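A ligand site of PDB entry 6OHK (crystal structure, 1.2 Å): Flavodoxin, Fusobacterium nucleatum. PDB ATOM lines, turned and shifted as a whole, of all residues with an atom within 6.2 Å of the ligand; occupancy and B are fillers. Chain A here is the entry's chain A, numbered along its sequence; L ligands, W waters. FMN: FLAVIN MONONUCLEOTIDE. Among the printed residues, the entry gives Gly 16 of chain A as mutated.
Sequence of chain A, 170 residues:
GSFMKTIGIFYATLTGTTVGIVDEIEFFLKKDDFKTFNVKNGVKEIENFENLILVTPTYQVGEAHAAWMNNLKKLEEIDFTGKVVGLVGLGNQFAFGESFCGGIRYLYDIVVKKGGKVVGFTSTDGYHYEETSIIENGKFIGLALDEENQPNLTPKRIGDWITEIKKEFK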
ATOM      1  N   ALA A  12     -19.445  21.702  12.678  1.00  0.00           N
ATOM      2  CA  ALA A  12     -18.138  21.753  12.051  1.00  0.00           C
ATOM      3  C   ALA A  12     -18.284  22.568  10.783  1.00  0.00           C
ATOM      4  O   ALA A  12     -19.366  22.684  10.231  1.00  0.00           O
ATOM      5  CB  ALA A  12     -17.639  20.352  11.716  1.00  0.00           C
ATOM      6  N   THR A  13     -17.155  23.068  10.284  1.00  0.00           N
ATOM      7  CA  THR A  13     -17.163  23.850   9.031  1.00  0.00           C
ATOM      8  C   THR A  13     -15.821  23.720   8.345  1.00  0.00           C
ATOM      9  O   THR A  13     -14.788  23.675   9.023  1.00  0.00           O
ATOM     10  CB  THR A  13     -17.500  25.319   9.294  1.00  0.00           C
ATOM     11  OG1 THR A  13     -17.677  26.013   8.053  1.00  0.00           O
ATOM     12  CG2 THR A  13     -16.400  26.019  10.066  1.00  0.00           C
ATOM     13  N   LEU A  14     -15.828  23.659   7.011  1.00  0.00           N
ATOM     14  CA  LEU A  14     -14.572  23.812   6.262  1.00  0.00           C
ATOM     15  C   LEU A  14     -14.400  25.247   5.770  1.00  0.00           C
ATOM     16  O   LEU A  14     -13.377  25.883   6.057  1.00  0.00           O
ATOM     17  CB  LEU A  14     -14.510  22.847   5.089  1.00  0.00           C
ATOM     18  CG  LEU A  14     -13.229  22.928   4.261  1.00  0.00           C
ATOM     19  CD1 LEU A  14     -11.996  22.509   5.056  1.00  0.00           C
ATOM     20  CD2 LEU A  14     -13.388  22.105   2.981  1.00  0.00           C
ATOM     21  N   THR A  15     -15.379  25.763   5.031  1.00  0.00           N
ATOM     22  CA  THR A  15     -15.242  27.077   4.431  1.00  0.00           C
ATOM     23  C   THR A  15     -16.115  28.155   5.027  1.00  0.00           C
ATOM     24  O   THR A  15     -16.147  29.279   4.479  1.00  0.00           O
ATOM     25  CB  THR A  15     -15.389  26.991   2.901  1.00  0.00           C
ATOM     26  OG1 THR A  15     -16.571  26.267   2.523  1.00  0.00           O
ATOM     27  CG2 THR A  15     -14.190  26.326   2.275  1.00  0.00           C
ATOM     28  N   GLY A  16     -16.798  27.899   6.143  1.00  0.00           N
ATOM     29  CA  GLY A  16     -17.472  28.929   6.886  1.00  0.00           C
ATOM     30  C   GLY A  16     -18.948  29.020   6.702  1.00  0.00           C
ATOM     31  O   GLY A  16     -19.607  29.724   7.487  1.00  0.00           O
ATOM     32  N   THR A  17     -19.532  28.336   5.737  1.00  0.00           N
ATOM     33  CA  THR A  17     -20.961  28.498   5.495  1.00  0.00           C
ATOM     34  C   THR A  17     -21.752  28.067   6.719  1.00  0.00           C
ATOM     35  O   THR A  17     -22.727  28.712   7.126  1.00  0.00           O
ATOM     36  CB  THR A  17     -21.402  27.663   4.301  1.00  0.00           C
ATOM     37  OG1 THR A  17     -20.531  27.880   3.182  1.00  0.00           O
ATOM     38  CG2 THR A  17     -22.809  28.015   3.888  1.00  0.00           C
ATOM     39  N   THR A  18     -21.344  26.960   7.326  1.00  0.00           N
ATOM     40  CA  THR A  18     -22.056  26.420   8.469  1.00  0.00           C
ATOM     41  C   THR A  18     -22.069  27.413   9.633  1.00  0.00           C
ATOM     42  O   THR A  18     -23.045  27.417  10.412  1.00  0.00           O
ATOM     43  CB  THR A  18     -21.436  25.077   8.866  1.00  0.00           C
ATOM     44  OG1 THR A  18     -21.575  24.150   7.799  1.00  0.00           O
ATOM     45  CG2 THR A  18     -22.169  24.479  10.027  1.00  0.00           C
ATOM     46  N   VAL A  19     -21.033  28.213   9.795  1.00  0.00           N
ATOM     47  CA  VAL A  19     -21.003  29.204  10.874  1.00  0.00           C
ATOM     48  C   VAL A  19     -22.188  30.136  10.773  1.00  0.00           C
ATOM     49  O   VAL A  19     -22.821  30.496  11.773  1.00  0.00           O
ATOM     50  CB  VAL A  19     -19.661  29.987  10.858  1.00  0.00           C
ATOM     51  CG1 VAL A  19     -19.670  31.160  11.860  1.00  0.00           C
ATOM     52  CG2 VAL A  19     -18.499  29.063  11.118  1.00  0.00           C
ATOM     53  N   PRO A  57     -21.867  20.273   7.394  1.00  0.00           N
ATOM     54  CA  PRO A  57     -21.846  20.210   5.941  1.00  0.00           C
ATOM     55  C   PRO A  57     -21.477  18.806   5.486  1.00  0.00           C
ATOM     56  O   PRO A  57     -21.063  17.957   6.252  1.00  0.00           O
ATOM     57  CB  PRO A  57     -20.766  21.224   5.574  1.00  0.00           C
ATOM     58  CG  PRO A  57     -19.766  21.095   6.719  1.00  0.00           C
ATOM     59  CD  PRO A  57     -20.631  20.865   7.947  1.00  0.00           C
ATOM     60  N   THR A  58     -21.607  18.570   4.189  1.00  0.00           N
ATOM     61  CA  THR A  58     -21.337  17.262   3.604  1.00  0.00           C
ATOM     62  C   THR A  58     -20.134  17.373   2.674  1.00  0.00           C
ATOM     63  O   THR A  58     -20.021  18.325   1.894  1.00  0.00           O
ATOM     64  CB  THR A  58     -22.523  16.846   2.770  1.00  0.00           C
ATOM     65  OG1 THR A  58     -23.737  17.157   3.459  1.00  0.00           O
ATOM     66  CG2 THR A  58     -22.455  15.404   2.320  1.00  0.00           C
ATOM     67  N   TYR A  59     -19.267  16.367   2.758  1.00  0.00           N
ATOM     68  CA  TYR A  59     -18.090  16.282   1.922  1.00  0.00           C
ATOM     69  C   TYR A  59     -17.878  14.815   1.580  1.00  0.00           C
ATOM     70  O   TYR A  59     -18.513  13.913   2.130  1.00  0.00           O
ATOM     71  CB  TYR A  59     -16.855  16.849   2.651  1.00  0.00           C
ATOM     72  CG  TYR A  59     -16.876  18.356   2.734  1.00  0.00           C
ATOM     73  CD1 TYR A  59     -16.585  19.113   1.613  1.00  0.00           C
ATOM     74  CD2 TYR A  59     -17.294  19.026   3.882  1.00  0.00           C
ATOM     75  CE1 TYR A  59     -16.653  20.472   1.657  1.00  0.00           C
ATOM     76  CE2 TYR A  59     -17.357  20.388   3.917  1.00  0.00           C
ATOM     77  CZ  TYR A  59     -17.027  21.112   2.811  1.00  0.00           C
ATOM     78  OH  TYR A  59     -17.077  22.486   2.735  1.00  0.00           O
ATOM     79  N   GLN A  60     -16.957  14.548   0.633  1.00  0.00           N
ATOM     80  CA  GLN A  60     -16.494  13.155   0.388  1.00  0.00           C
ATOM     81  C   GLN A  60     -17.648  12.185   0.098  1.00  0.00           C
ATOM     82  O   GLN A  60     -17.739  11.093   0.663  1.00  0.00           O
ATOM     83  CB  GLN A  60     -15.674  12.654   1.583  1.00  0.00           C
ATOM     84  CG  GLN A  60     -14.399  13.390   1.840  1.00  0.00           C
ATOM     85  CD  GLN A  60     -13.311  13.045   0.840  1.00  0.00           C
ATOM     86  OE1 GLN A  60     -13.157  11.890   0.450  1.00  0.00           O
ATOM     87  NE2 GLN A  60     -12.553  14.051   0.412  1.00  0.00           N
ATOM     88  N   VAL A  61     -18.546  12.600  -0.782  1.00  0.00           N
ATOM     89  CA  VAL A  61     -19.629  11.731  -1.253  1.00  0.00           C
ATOM     90  C   VAL A  61     -20.498  11.297  -0.090  1.00  0.00           C
ATOM     91  O   VAL A  61     -20.695  10.102   0.179  1.00  0.00           O
ATOM     92  CB  VAL A  61     -19.106  10.515  -2.053  1.00  0.00           C
ATOM     93  CG1 VAL A  61     -20.221   9.975  -2.930  1.00  0.00           C
ATOM     94  CG2 VAL A  61     -17.899  10.889  -2.897  1.00  0.00           C
ATOM     95  N   GLY A  62     -21.080  12.273   0.585  1.00  0.00           N
ATOM     96  CA  GLY A  62     -22.081  12.006   1.569  1.00  0.00           C
ATOM     97  C   GLY A  62     -21.581  11.818   2.991  1.00  0.00           C
ATOM     98  O   GLY A  62     -22.359  11.443   3.862  1.00  0.00           O
ATOM     99  N   GLU A  63     -20.322  12.115   3.258  1.00  0.00           N
ATOM    100  CA  GLU A  63     -19.821  12.064   4.626  1.00  0.00           C
ATOM    101  C   GLU A  63     -20.087  13.381   5.339  1.00  0.00           C
ATOM    102  O   GLU A  63     -20.333  14.421   4.728  1.00  0.00           O
ATOM    103  CB  GLU A  63     -18.315  11.795   4.650  1.00  0.00           C
ATOM    104  CG  GLU A  63     -17.954  10.418   4.149  1.00  0.00           C
ATOM    105  CD  GLU A  63     -16.469  10.108   4.282  1.00  0.00           C
ATOM    106  OE1 GLU A  63     -15.692  10.970   4.740  1.00  0.00           O
ATOM    107  OE2 GLU A  63     -16.062   8.988   3.892  1.00  0.00           O
ATOM    108  N   HIS A  65     -18.442  16.372   7.866  1.00  0.00           N
ATOM    109  CA  HIS A  65     -17.129  16.993   7.939  1.00  0.00           C
ATOM    110  C   HIS A  65     -16.168  16.083   8.690  1.00  0.00           C
ATOM    111  O   HIS A  65     -16.576  15.335   9.579  1.00  0.00           O
ATOM    112  CB  HIS A  65     -17.299  18.321   8.668  1.00  0.00           C
ATOM    113  CG  HIS A  65     -16.055  19.160   8.778  1.00  0.00           C
ATOM    114  ND1 HIS A  65     -15.046  18.904   9.680  1.00  0.00           N
ATOM    115  CD2 HIS A  65     -15.709  20.279   8.113  1.00  0.00           C
ATOM    116  CE1 HIS A  65     -14.123  19.829   9.552  1.00  0.00           C
ATOM    117  NE2 HIS A  65     -14.494  20.669   8.602  1.00  0.00           N
ATOM    118  N   LEU A  90     -25.890  20.752   5.681  1.00  0.00           N
ATOM    119  CA  LEU A  90     -25.675  21.685   4.568  1.00  0.00           C
ATOM    120  C   LEU A  90     -25.105  20.895   3.418  1.00  0.00           C
ATOM    121  O   LEU A  90     -24.260  20.023   3.617  1.00  0.00           O
ATOM    122  CB  LEU A  90     -24.675  22.754   4.915  1.00  0.00           C
ATOM    123  CG  LEU A  90     -25.168  23.900   5.786  1.00  0.00           C
ATOM    124  CD1 LEU A  90     -25.178  23.515   7.239  1.00  0.00           C
ATOM    125  CD2 LEU A  90     -24.242  25.055   5.598  1.00  0.00           C
ATOM    126  N   GLY A  91     -25.588  21.200   2.215  1.00  0.00           N
ATOM    127  CA  GLY A  91     -25.081  20.533   1.027  1.00  0.00           C
ATOM    128  C   GLY A  91     -25.466  21.277  -0.232  1.00  0.00           C
ATOM    129  O   GLY A  91     -25.898  22.420  -0.194  1.00  0.00           O
ATOM    130  N   ASN A  92     -25.281  20.596  -1.371  1.00  0.00           N
ATOM    131  CA  ASN A  92     -25.632  21.135  -2.686  1.00  0.00           C
ATOM    132  C   ASN A  92     -26.414  20.057  -3.424  1.00  0.00           C
ATOM    133  O   ASN A  92     -25.847  19.062  -3.858  1.00  0.00           O
ATOM    134  CB  ASN A  92     -24.365  21.540  -3.434  1.00  0.00           C
ATOM    135  CG  ASN A  92     -24.658  22.061  -4.839  1.00  0.00           C
ATOM    136  OD1 ASN A  92     -25.648  21.728  -5.450  1.00  0.00           O
ATOM    137  ND2 ASN A  92     -23.776  22.916  -5.334  1.00  0.00           N
ATOM    138  N   GLN A  93     -27.721  20.241  -3.533  1.00  0.00           N
ATOM    139  CA  GLN A  93     -28.567  19.141  -3.988  1.00  0.00           C
ATOM    140  C   GLN A  93     -28.405  18.880  -5.475  1.00  0.00           C
ATOM    141  O   GLN A  93     -28.713  17.773  -5.923  1.00  0.00           O
ATOM    142  CB  GLN A  93     -30.032  19.410  -3.643  1.00  0.00           C
ATOM    143  CG  GLN A  93     -30.642  20.584  -4.443  1.00  0.00           C
ATOM    144  CD  GLN A  93     -31.833  21.176  -3.737  1.00  0.00           C
ATOM    145  OE1 GLN A  93     -32.977  20.751  -3.971  1.00  0.00           O
ATOM    146  NE2 GLN A  93     -31.579  22.114  -2.850  1.00  0.00           N
ATOM    147  N   PHE A  96     -24.686  17.217  -6.119  1.00  0.00           N
ATOM    148  CA  PHE A  96     -24.536  15.938  -5.436  1.00  0.00           C
ATOM    149  C   PHE A  96     -25.893  15.264  -5.381  1.00  0.00           C
ATOM    150  O   PHE A  96     -26.512  15.136  -4.319  1.00  0.00           O
ATOM    151  CB  PHE A  96     -23.922  16.153  -4.059  1.00  0.00           C
ATOM    152  CG  PHE A  96     -22.597  16.829  -4.145  1.00  0.00           C
ATOM    153  CD1 PHE A  96     -21.467  16.126  -4.521  1.00  0.00           C
ATOM    154  CD2 PHE A  96     -22.479  18.192  -3.946  1.00  0.00           C
ATOM    155  CE1 PHE A  96     -20.251  16.770  -4.662  1.00  0.00           C
ATOM    156  CE2 PHE A  96     -21.259  18.836  -4.109  1.00  0.00           C
ATOM    157  CZ  PHE A  96     -20.153  18.109  -4.471  1.00  0.00           C
ATOM    158  N   SER A  99     -26.082  12.333  -2.886  1.00  0.00           N
ATOM    159  CA  SER A  99     -25.464  12.442  -1.553  1.00  0.00           C
ATOM    160  C   SER A  99     -25.794  13.754  -0.882  1.00  0.00           C
ATOM    161  O   SER A  99     -25.039  14.208  -0.014  1.00  0.00           O
ATOM    162  CB  SER A  99     -23.970  12.196  -1.603  1.00  0.00           C
ATOM    163  OG  SER A  99     -23.281  13.152  -2.396  1.00  0.00           O
ATOM    164  N   PHE A 100     -26.895  14.384  -1.233  1.00  0.00           N
ATOM    165  CA  PHE A 100     -27.232  15.674  -0.659  1.00  0.00           C
ATOM    166  C   PHE A 100     -27.456  15.572   0.833  1.00  0.00           C
ATOM    167  O   PHE A 100     -28.313  14.824   1.303  1.00  0.00           O
ATOM    168  CB  PHE A 100     -28.493  16.201  -1.329  1.00  0.00           C
ATOM    169  CG  PHE A 100     -29.045  17.470  -0.726  1.00  0.00           C
ATOM    170  CD1 PHE A 100     -28.284  18.624  -0.663  1.00  0.00           C
ATOM    171  CD2 PHE A 100     -30.342  17.531  -0.267  1.00  0.00           C
ATOM    172  CE1 PHE A 100     -28.789  19.788  -0.138  1.00  0.00           C
ATOM    173  CE2 PHE A 100     -30.842  18.675   0.268  1.00  0.00           C
ATOM    174  CZ  PHE A 100     -30.073  19.799   0.326  1.00  0.00           C
ATOM    175  N   CYS A 101     -26.698  16.370   1.590  1.00  0.00           N
ATOM    176  CA  CYS A 101     -26.773  16.366   3.037  1.00  0.00           C
ATOM    177  C   CYS A 101     -26.572  14.984   3.634  1.00  0.00           C
ATOM    178  O   CYS A 101     -27.076  14.680   4.713  1.00  0.00           O
ATOM    179  CB  CYS A 101     -28.065  17.018   3.576  1.00  0.00           C
ATOM    180  SG  CYS A 101     -28.108  18.786   3.396  1.00  0.00           S
ATOM    181  N   GLY A 102     -25.802  14.143   2.962  1.00  0.00           N
ATOM    182  CA  GLY A 102     -25.620  12.777   3.430  1.00  0.00           C
ATOM    183  C   GLY A 102     -24.958  12.658   4.780  1.00  0.00           C
ATOM    184  O   GLY A 102     -25.103  11.621   5.438  1.00  0.00           O
ATOM    185  N   GLU A 147     -27.254  26.366   0.770  1.00  0.00           N
ATOM    186  CA  GLU A 147     -26.908  27.776   0.663  1.00  0.00           C
ATOM    187  C   GLU A 147     -26.408  28.141  -0.718  1.00  0.00           C
ATOM    188  O   GLU A 147     -26.389  29.330  -1.066  1.00  0.00           O
ATOM    189  CB  GLU A 147     -25.855  28.127   1.723  1.00  0.00           C
ATOM    190  CG  GLU A 147     -26.427  28.312   3.098  1.00  0.00           C
ATOM    191  CD  GLU A 147     -27.145  29.650   3.188  1.00  0.00           C
ATOM    192  OE1 GLU A 147     -26.530  30.705   2.858  1.00  0.00           O
ATOM    193  OE2 GLU A 147     -28.327  29.688   3.493  1.00  0.00           O
ATOM    194  N   GLU A 148     -25.966  27.168  -1.506  1.00  0.00           N
ATOM    195  CA  GLU A 148     -25.485  27.466  -2.847  1.00  0.00           C
ATOM    196  C   GLU A 148     -26.647  27.745  -3.777  1.00  0.00           C
ATOM    197  O   GLU A 148     -26.553  28.646  -4.633  1.00  0.00           O
ATOM    198  CB  GLU A 148     -24.633  26.299  -3.350  1.00  0.00           C
ATOM    199  CG  GLU A 148     -23.332  26.120  -2.508  1.00  0.00           C
ATOM    200  CD  GLU A 148     -22.414  25.081  -3.100  1.00  0.00           C
ATOM    201  OE1 GLU A 148     -22.033  25.248  -4.276  1.00  0.00           O
ATOM    202  OE2 GLU A 148     -22.099  24.087  -2.418  1.00  0.00           O
HETATM  203  N1  FMN L   1     -22.811  18.685  -0.594  1.00  0.00           N
HETATM  204  C2  FMN L   1     -23.673  17.585  -0.507  1.00  0.00           C
HETATM  205  O2  FMN L   1     -24.835  17.711  -0.310  1.00  0.00           O
HETATM  206  N3  FMN L   1     -23.097  16.274  -0.691  1.00  0.00           N
HETATM  207  C4  FMN L   1     -21.772  16.020  -0.949  1.00  0.00           C
HETATM  208  O4  FMN L   1     -21.420  14.871  -1.077  1.00  0.00           O
HETATM  209  C4A FMN L   1     -20.937  17.162  -1.052  1.00  0.00           C
HETATM  210  N5  FMN L   1     -19.579  16.973  -1.329  1.00  0.00           N
HETATM  211  C5A FMN L   1     -18.804  18.157  -1.480  1.00  0.00           C
HETATM  212  C6  FMN L   1     -17.461  18.021  -1.885  1.00  0.00           C
HETATM  213  C7  FMN L   1     -16.675  19.143  -2.037  1.00  0.00           C
HETATM  214  C7M FMN L   1     -15.208  18.850  -2.400  1.00  0.00           C
HETATM  215  C8  FMN L   1     -17.224  20.410  -1.886  1.00  0.00           C
HETATM  216  C8M FMN L   1     -16.304  21.611  -2.015  1.00  0.00           C
HETATM  217  C9  FMN L   1     -18.549  20.544  -1.483  1.00  0.00           C
HETATM  218  C9A FMN L   1     -19.334  19.424  -1.318  1.00  0.00           C
HETATM  219  N10 FMN L   1     -20.720  19.593  -0.905  1.00  0.00           N
HETATM  220  C10 FMN L   1     -21.489  18.453  -0.846  1.00  0.00           C
HETATM  221  C1' FMN L   1     -21.291  20.921  -0.688  1.00  0.00           C
HETATM  222  C2' FMN L   1     -20.887  21.489   0.703  1.00  0.00           C
HETATM  223  O2' FMN L   1     -21.319  20.656   1.772  1.00  0.00           O
HETATM  224  C3' FMN L   1     -21.574  22.862   0.885  1.00  0.00           C
HETATM  225  O3' FMN L   1     -20.957  23.755  -0.034  1.00  0.00           O
HETATM  226  C4' FMN L   1     -21.546  23.452   2.291  1.00  0.00           C
HETATM  227  O4' FMN L   1     -22.335  24.637   2.288  1.00  0.00           O
HETATM  228  C5' FMN L   1     -20.132  23.796   2.769  1.00  0.00           C
HETATM  229  O5' FMN L   1     -20.228  24.159   4.134  1.00  0.00           O
HETATM  230  P   FMN L   1     -18.960  24.805   4.885  1.00  0.00           P
HETATM  231  O1P FMN L   1     -19.477  25.059   6.280  1.00  0.00           O
HETATM  232  O2P FMN L   1     -17.788  23.880   4.857  1.00  0.00           O
HETATM  233  O3P FMN L   1     -18.622  26.114   4.153  1.00  0.00           O
HETATM  234  O   HOH W   1     -13.989  23.647  -0.491  1.00  0.00           O
HETATM  235  O   HOH W   2     -21.603  26.936   0.758  1.00  0.00           O
HETATM  236  O   HOH W   3     -25.063  24.553   1.476  1.00  0.00           O
HETATM  237  O   HOH W   4     -18.585  14.643  -2.636  1.00  0.00           O
HETATM  238  O   HOH W   5     -18.459  24.553  -0.956  1.00  0.00           O
HETATM  239  O   HOH W   6     -14.665  16.252  -0.426  1.00  0.00           O
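OG1 of Thr 13 lies within hydrogen-bond range of O1P of the ligand (2.7 Å). OG of Ser 99 is in hydrogen-bond range of O4 of the ligand (2.9 Å). A nitrogen (N3) of the ligand is in hydrogen-bond range of the backbone carbonyl oxygen of Ser 99 (2.9 Å). The side-chain hydroxyl of Tyr 59 is in hydrogen-bond range of an oxygen (O2P) of the ligand, at 2.6 Å. An oxygen (O3P) of the ligand is in hydrogen-bond range of the backbone NH (N) of Thr 17 (2.9 Å). OE2 of Glu 148 is in hydrogen-bond range of O3' of the ligand, at 2.7 Å. An oxygen (O3P) of the ligand lies within hydrogen-bond range of the side-chain hydroxyl (OG1) of Thr 15, 2.6 Å away. The backbone NH (N) of Thr 15 is in hydrogen-bond range of an oxygen (O2P) of the ligand (3.1 Å). O of Thr 58 is in hydrogen-bond range of O2' of the ligand (2.7 Å). The side-chain hydroxyl (OG1) of Thr 17 is in hydrogen-bond range of an oxygen (O3P) of the ligand (2.8 Å). N of Leu 14 is in hydrogen-bond range of O2P of the ligand, at 2.9 Å. O2' of the ligand lies within hydrogen-bond range of N of Thr 58 (3.2 Å). The backbone NH (N) of Cys 101 lies within hydrogen-bond range of an oxygen (O2) of the ligand (3.0 Å). An oxygen (O1P) of the ligand lies within hydrogen-bond range of the backbone NH (N) of Thr 18, 2.9 Å away. An oxygen (O2) of the ligand is in hydrogen-bond range of the backbone NH (N) of Asn 92 (3.1 Å). The side-chain hydroxyl (OG1) of Thr 18 is in hydrogen-bond range of an oxygen (O1P) of the ligand (2.7 Å). The backbone NH (N) of Gly 16 lies within hydrogen-bond range of an oxygen (O3P) of the ligand. An oxygen (O4) of the ligand is in hydrogen-bond range of the backbone NH (N) of Gly 62 (3.1 Å).
N of Gly 16 lies within hydrogen-bond range of OG1 of Thr 13 (2.8 Å). The side-chain amide nitrogen (ND2) of Asn 92 lies within hydrogen-bond range of the side-chain carboxylate (OE1) of Glu 148, at 3.1 Å. A ring nitrogen (NE2) of His 65 sits at hydrogen-bond distance from the backbone carbonyl oxygen (O) of Thr 13, at 3.0 Å. The backbone NH (N) of Leu 90 sits close to the side-chain sulfur (SG) of Cys 101, 3.7 Å away. The side-chain hydroxyl (OG1) of Thr 58 is in hydrogen-bond range of the backbone carbonyl oxygen (O) of Leu 90, at 2.9 Å. N of Gly 91 is in hydrogen-bond range of SG of Cys 101 (3.7 Å). O of Pro 57 sits at hydrogen-bond distance from N of His 65 (3.5 Å).
Merely in contact with the ligand: Gly 91 (3.1 Å), Phe 100 (3.2 Å), Phe 96 (3.3 Å), Pro 57 (3.3 Å), Leu 90 (3.5 Å) and Val 61 (3.6 Å). Hydrophobic or aromatic side chains within 4 Å of the ligand: Leu 14, Pro 57, Tyr 59, Leu 90, Phe 96 and Phe 100. Within 4 Å of the ligand: Thr 13, Leu 14, Thr 15, Gly 16, Thr 17, Thr 18, Pro 57, Thr 58, Tyr 59, Val 61, Gly 62, Leu 90, Gly 91, Asn 92, Phe 96, Ser 99, Phe 100, Cys 101 and Glu 148.
Water W3 lies within hydrogen-bond range of the backbone carbonyl oxygen of Gly 91 (2.8 Å), an oxygen (O4') of the ligand (2.8 Å) and the backbone NH of Glu 147 (2.9 Å). Water W4 lies within hydrogen-bond range of the backbone NH of Val 61 (2.8 Å) and a nitrogen (N5) of the ligand (2.9 Å). Water W2 bridges OG1 of Thr 17 (2.8 Å) and O4' of the ligand (2.9 Å).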
